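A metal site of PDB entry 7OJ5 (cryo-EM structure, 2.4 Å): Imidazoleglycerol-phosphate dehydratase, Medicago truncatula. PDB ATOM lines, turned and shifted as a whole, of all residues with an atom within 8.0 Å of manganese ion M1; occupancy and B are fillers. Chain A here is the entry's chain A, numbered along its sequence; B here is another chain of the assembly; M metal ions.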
ATOM      1  N   PHE A  44     -26.310 -24.541 -21.585  1.00  0.00           N
ATOM      2  CA  PHE A  44     -25.996 -23.269 -20.927  1.00  0.00           C
ATOM      3  C   PHE A  44     -24.523 -22.936 -21.041  1.00  0.00           C
ATOM      4  O   PHE A  44     -24.152 -21.757 -21.147  1.00  0.00           O
ATOM      5  CB  PHE A  44     -26.423 -23.309 -19.464  1.00  0.00           C
ATOM      6  CG  PHE A  44     -26.216 -22.006 -18.745  1.00  0.00           C
ATOM      7  CD1 PHE A  44     -27.133 -20.973 -18.876  1.00  0.00           C
ATOM      8  CD2 PHE A  44     -25.097 -21.802 -17.950  1.00  0.00           C
ATOM      9  CE1 PHE A  44     -26.938 -19.767 -18.228  1.00  0.00           C
ATOM     10  CE2 PHE A  44     -24.902 -20.596 -17.302  1.00  0.00           C
ATOM     11  CZ  PHE A  44     -25.821 -19.577 -17.437  1.00  0.00           C
ATOM     12  N   HIS A  47     -23.952 -21.319 -24.342  1.00  0.00           N
ATOM     13  CA  HIS A  47     -24.322 -19.917 -24.300  1.00  0.00           C
ATOM     14  C   HIS A  47     -23.208 -19.065 -23.703  1.00  0.00           C
ATOM     15  O   HIS A  47     -22.973 -17.937 -24.145  1.00  0.00           O
ATOM     16  CB  HIS A  47     -25.626 -19.747 -23.514  1.00  0.00           C
ATOM     17  CG  HIS A  47     -26.119 -18.337 -23.428  1.00  0.00           C
ATOM     18  ND1 HIS A  47     -26.263 -17.525 -24.530  1.00  0.00           N
ATOM     19  CD2 HIS A  47     -26.539 -17.596 -22.363  1.00  0.00           C
ATOM     20  CE1 HIS A  47     -26.734 -16.341 -24.151  1.00  0.00           C
ATOM     21  NE2 HIS A  47     -26.903 -16.366 -22.843  1.00  0.00           N
ATOM     22  N   MET A  48     -22.501 -19.600 -22.702  1.00  0.00           N
ATOM     23  CA  MET A  48     -21.421 -18.858 -22.068  1.00  0.00           C
ATOM     24  C   MET A  48     -20.207 -18.765 -22.981  1.00  0.00           C
ATOM     25  O   MET A  48     -19.546 -17.717 -23.035  1.00  0.00           O
ATOM     26  CB  MET A  48     -21.032 -19.513 -20.735  1.00  0.00           C
ATOM     27  CG  MET A  48     -21.945 -19.245 -19.524  1.00  0.00           C
ATOM     28  SD  MET A  48     -22.409 -17.544 -19.103  1.00  0.00           S
ATOM     29  CE  MET A  48     -23.827 -17.248 -20.174  1.00  0.00           C
ATOM     30  N   GLN A  51     -20.269 -15.964 -25.700  1.00  0.00           N
ATOM     31  CA  GLN A  51     -19.934 -14.611 -25.275  1.00  0.00           C
ATOM     32  C   GLN A  51     -18.435 -14.394 -25.209  1.00  0.00           C
ATOM     33  O   GLN A  51     -17.972 -13.256 -25.390  1.00  0.00           O
ATOM     34  CB  GLN A  51     -20.565 -14.317 -23.911  1.00  0.00           C
ATOM     35  CG  GLN A  51     -21.943 -14.907 -23.722  1.00  0.00           C
ATOM     36  CD  GLN A  51     -23.042 -13.927 -24.055  1.00  0.00           C
ATOM     37  OE1 GLN A  51     -22.777 -12.817 -24.495  1.00  0.00           O
ATOM     38  NE2 GLN A  51     -24.286 -14.344 -23.852  1.00  0.00           N
ATOM     39  N   LEU A 107     -23.942  -5.559 -15.847  1.00  0.00           N
ATOM     40  CA  LEU A 107     -25.076  -6.201 -16.536  1.00  0.00           C
ATOM     41  C   LEU A 107     -26.296  -5.994 -15.641  1.00  0.00           C
ATOM     42  O   LEU A 107     -26.555  -6.774 -14.726  1.00  0.00           O
ATOM     43  CB  LEU A 107     -24.812  -7.671 -16.806  1.00  0.00           C
ATOM     44  CG  LEU A 107     -25.381  -8.313 -18.080  1.00  0.00           C
ATOM     45  CD1 LEU A 107     -24.954  -9.772 -18.177  1.00  0.00           C
ATOM     46  CD2 LEU A 107     -26.897  -8.191 -18.171  1.00  0.00           C
ATOM     47  N   HIS A 169     -28.633 -15.588 -13.671  1.00  0.00           N
ATOM     48  CA  HIS A 169     -28.228 -15.504 -15.070  1.00  0.00           C
ATOM     49  C   HIS A 169     -27.347 -14.287 -15.323  1.00  0.00           C
ATOM     50  O   HIS A 169     -26.358 -14.374 -16.054  1.00  0.00           O
ATOM     51  CB  HIS A 169     -29.462 -15.484 -15.973  1.00  0.00           C
ATOM     52  CG  HIS A 169     -29.174 -15.608 -17.432  1.00  0.00           C
ATOM     53  ND1 HIS A 169     -29.571 -16.699 -18.183  1.00  0.00           N
ATOM     54  CD2 HIS A 169     -28.536 -14.778 -18.296  1.00  0.00           C
ATOM     55  CE1 HIS A 169     -29.184 -16.535 -19.432  1.00  0.00           C
ATOM     56  NE2 HIS A 169     -28.562 -15.377 -19.527  1.00  0.00           N
ATOM     57  N   HIS A 170     -27.707 -13.143 -14.727  1.00  0.00           N
ATOM     58  CA  HIS A 170     -26.945 -11.918 -14.962  1.00  0.00           C
ATOM     59  C   HIS A 170     -25.550 -11.992 -14.338  1.00  0.00           C
ATOM     60  O   HIS A 170     -24.586 -11.497 -14.923  1.00  0.00           O
ATOM     61  CB  HIS A 170     -27.712 -10.711 -14.414  1.00  0.00           C
ATOM     62  CG  HIS A 170     -28.955 -10.384 -15.196  1.00  0.00           C
ATOM     63  ND1 HIS A 170     -29.859  -9.438 -14.778  1.00  0.00           N
ATOM     64  CD2 HIS A 170     -29.427 -10.874 -16.360  1.00  0.00           C
ATOM     65  CE1 HIS A 170     -30.846  -9.362 -15.655  1.00  0.00           C
ATOM     66  NE2 HIS A 170     -30.601 -10.220 -16.624  1.00  0.00           N
ATOM     67  N   GLU A 173     -23.190 -14.504 -16.444  1.00  0.00           N
ATOM     68  CA  GLU A 173     -22.911 -14.085 -17.811  1.00  0.00           C
ATOM     69  C   GLU A 173     -22.190 -12.736 -17.832  1.00  0.00           C
ATOM     70  O   GLU A 173     -21.516 -12.401 -18.811  1.00  0.00           O
ATOM     71  CB  GLU A 173     -24.222 -14.098 -18.612  1.00  0.00           C
ATOM     72  CG  GLU A 173     -24.293 -13.362 -19.930  1.00  0.00           C
ATOM     73  CD  GLU A 173     -25.634 -13.606 -20.624  1.00  0.00           C
ATOM     74  OE1 GLU A 173     -25.867 -14.767 -21.036  1.00  0.00           O
ATOM     75  OE2 GLU A 173     -26.455 -12.683 -20.767  1.00  0.00           O
ATOM     76  N   ALA A 174     -22.258 -11.981 -16.735  1.00  0.00           N
ATOM     77  CA  ALA A 174     -21.380 -10.827 -16.580  1.00  0.00           C
ATOM     78  C   ALA A 174     -19.948 -11.240 -16.270  1.00  0.00           C
ATOM     79  O   ALA A 174     -19.000 -10.536 -16.638  1.00  0.00           O
ATOM     80  CB  ALA A 174     -21.902  -9.891 -15.492  1.00  0.00           C
ATOM     81  N   LYS A 177     -18.198 -12.096 -19.571  1.00  0.00           N
ATOM     82  CA  LYS A 177     -17.890 -10.907 -20.357  1.00  0.00           C
ATOM     83  C   LYS A 177     -16.622 -10.220 -19.865  1.00  0.00           C
ATOM     84  O   LYS A 177     -15.783  -9.802 -20.667  1.00  0.00           O
ATOM     85  CB  LYS A 177     -19.061  -9.932 -20.308  1.00  0.00           C
ATOM     86  CG  LYS A 177     -20.202 -10.264 -21.247  1.00  0.00           C
ATOM     87  CD  LYS A 177     -21.350  -9.278 -21.080  1.00  0.00           C
ATOM     88  CE  LYS A 177     -22.603  -9.736 -21.806  1.00  0.00           C
ATOM     89  NZ  LYS A 177     -23.475  -8.590 -22.159  1.00  0.00           N
ATOM     90  N   GLU B  21     -32.640 -14.607 -30.621  1.00  0.00           N
ATOM     91  CA  GLU B  21     -33.078 -15.576 -29.615  1.00  0.00           C
ATOM     92  C   GLU B  21     -34.574 -15.816 -29.597  1.00  0.00           C
ATOM     93  O   GLU B  21     -34.990 -16.934 -29.286  1.00  0.00           O
ATOM     94  CB  GLU B  21     -32.627 -15.114 -28.225  1.00  0.00           C
ATOM     95  CG  GLU B  21     -31.168 -14.716 -28.134  1.00  0.00           C
ATOM     96  CD  GLU B  21     -30.782 -14.200 -26.757  1.00  0.00           C
ATOM     97  OE1 GLU B  21     -31.502 -13.331 -26.229  1.00  0.00           O
ATOM     98  OE2 GLU B  21     -29.771 -14.679 -26.201  1.00  0.00           O
ATOM     99  N   ASP B  67     -35.485 -19.799 -27.562  1.00  0.00           N
ATOM    100  CA  ASP B  67     -34.492 -20.801 -27.161  1.00  0.00           C
ATOM    101  C   ASP B  67     -34.724 -21.220 -25.700  1.00  0.00           C
ATOM    102  O   ASP B  67     -33.937 -20.951 -24.798  1.00  0.00           O
ATOM    103  CB  ASP B  67     -33.081 -20.266 -27.375  1.00  0.00           C
ATOM    104  CG  ASP B  67     -32.886 -18.876 -26.787  1.00  0.00           C
ATOM    105  OD1 ASP B  67     -33.815 -18.352 -26.150  1.00  0.00           O
ATOM    106  OD2 ASP B  67     -31.789 -18.308 -26.975  1.00  0.00           O
ATOM    107  N   ILE B  70     -32.191 -23.617 -23.478  1.00  0.00           N
ATOM    108  CA  ILE B  70     -31.185 -23.096 -22.561  1.00  0.00           C
ATOM    109  C   ILE B  70     -31.813 -22.674 -21.237  1.00  0.00           C
ATOM    110  O   ILE B  70     -31.430 -23.155 -20.172  1.00  0.00           O
ATOM    111  CB  ILE B  70     -30.428 -21.920 -23.220  1.00  0.00           C
ATOM    112  CG1 ILE B  70     -29.652 -22.389 -24.453  1.00  0.00           C
ATOM    113  CG2 ILE B  70     -29.499 -21.250 -22.224  1.00  0.00           C
ATOM    114  CD1 ILE B  70     -29.364 -21.296 -25.452  1.00  0.00           C
ATOM    115  N   ASP B  71     -32.779 -21.770 -21.302  1.00  0.00           N
ATOM    116  CA  ASP B  71     -33.443 -21.226 -20.122  1.00  0.00           C
ATOM    117  C   ASP B  71     -34.718 -20.535 -20.569  1.00  0.00           C
ATOM    118  O   ASP B  71     -34.949 -20.328 -21.769  1.00  0.00           O
ATOM    119  CB  ASP B  71     -32.530 -20.254 -19.369  1.00  0.00           C
ATOM    120  CG  ASP B  71     -32.814 -20.219 -17.884  1.00  0.00           C
ATOM    121  OD1 ASP B  71     -33.815 -20.838 -17.454  1.00  0.00           O
ATOM    122  OD2 ASP B  71     -32.060 -19.551 -17.146  1.00  0.00           O
ATOM    123  N   HIS B  73     -35.183 -17.492 -19.438  1.00  0.00           N
ATOM    124  CA  HIS B  73     -34.855 -16.094 -19.157  1.00  0.00           C
ATOM    125  C   HIS B  73     -35.078 -15.202 -20.366  1.00  0.00           C
ATOM    126  O   HIS B  73     -35.723 -14.155 -20.262  1.00  0.00           O
ATOM    127  CB  HIS B  73     -33.399 -16.006 -18.669  1.00  0.00           C
ATOM    128  CG  HIS B  73     -32.977 -14.625 -18.273  1.00  0.00           C
ATOM    129  ND1 HIS B  73     -32.750 -14.258 -16.965  1.00  0.00           N
ATOM    130  CD2 HIS B  73     -32.711 -13.518 -19.011  1.00  0.00           C
ATOM    131  CE1 HIS B  73     -32.386 -12.993 -16.915  1.00  0.00           C
ATOM    132  NE2 HIS B  73     -32.347 -12.527 -18.143  1.00  0.00           N
ATOM    133  N   HIS B  74     -34.538 -15.600 -21.523  1.00  0.00           N
ATOM    134  CA  HIS B  74     -34.585 -14.721 -22.692  1.00  0.00           C
ATOM    135  C   HIS B  74     -36.015 -14.580 -23.227  1.00  0.00           C
ATOM    136  O   HIS B  74     -36.401 -13.506 -23.693  1.00  0.00           O
ATOM    137  CB  HIS B  74     -33.646 -15.230 -23.783  1.00  0.00           C
ATOM    138  CG  HIS B  74     -32.194 -15.231 -23.373  1.00  0.00           C
ATOM    139  ND1 HIS B  74     -31.351 -16.286 -23.661  1.00  0.00           N
ATOM    140  CD2 HIS B  74     -31.454 -14.320 -22.712  1.00  0.00           C
ATOM    141  CE1 HIS B  74     -30.142 -16.015 -23.183  1.00  0.00           C
ATOM    142  NE2 HIS B  74     -30.173 -14.827 -22.602  1.00  0.00           N
ATOM    143  N   GLU B  77     -38.046 -12.274 -20.690  1.00  0.00           N
ATOM    144  CA  GLU B  77     -37.675 -10.869 -20.784  1.00  0.00           C
ATOM    145  C   GLU B  77     -38.269 -10.215 -22.031  1.00  0.00           C
ATOM    146  O   GLU B  77     -38.747  -9.071 -21.974  1.00  0.00           O
ATOM    147  CB  GLU B  77     -36.151 -10.722 -20.768  1.00  0.00           C
ATOM    148  CG  GLU B  77     -35.642  -9.301 -20.925  1.00  0.00           C
ATOM    149  CD  GLU B  77     -34.188  -9.137 -20.528  1.00  0.00           C
ATOM    150  OE1 GLU B  77     -33.566 -10.135 -20.080  1.00  0.00           O
ATOM    151  OE2 GLU B  77     -33.656  -8.021 -20.680  1.00  0.00           O
HETATM  152 MN    MN M   1     -27.943 -14.506 -21.629  1.00  0.00          MN
HETATM  153 MN    MN M   2     -32.201 -10.235 -18.284  1.00  0.00          MN
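The nearest printed residue that does not touch manganese ion M1 is Gln 51 (4.3 Å).
The side-chain carboxylate (OE2) of Glu 21 of chain B sits close to a ring nitrogen (ND1) of His 74 of chain B (3.4 Å). The side-chain carboxylate (OE1) of Glu 173 sits close to the side-chain amide nitrogen (NE2) of Gln 51 (3.3 Å). A ring nitrogen (NE2) of His 47 lies close to the side-chain amide nitrogen (NE2) of Gln 51, 3.5 Å away.
OE1 of Glu 173 binds manganese ion M1 (2.2 Å). NE2 of His 169 binds manganese ion M1 (2.4 Å). Manganese ion M1 is bound by NE2 of His 47, at 2.5 Å. NE2 of His 74 of chain B is bound to manganese ion M1, at 2.5 Å. OE2 of Glu 173 binds manganese ion M1, 2.5 Å away. Manganese ion M1 has five donor atoms within binding distance.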
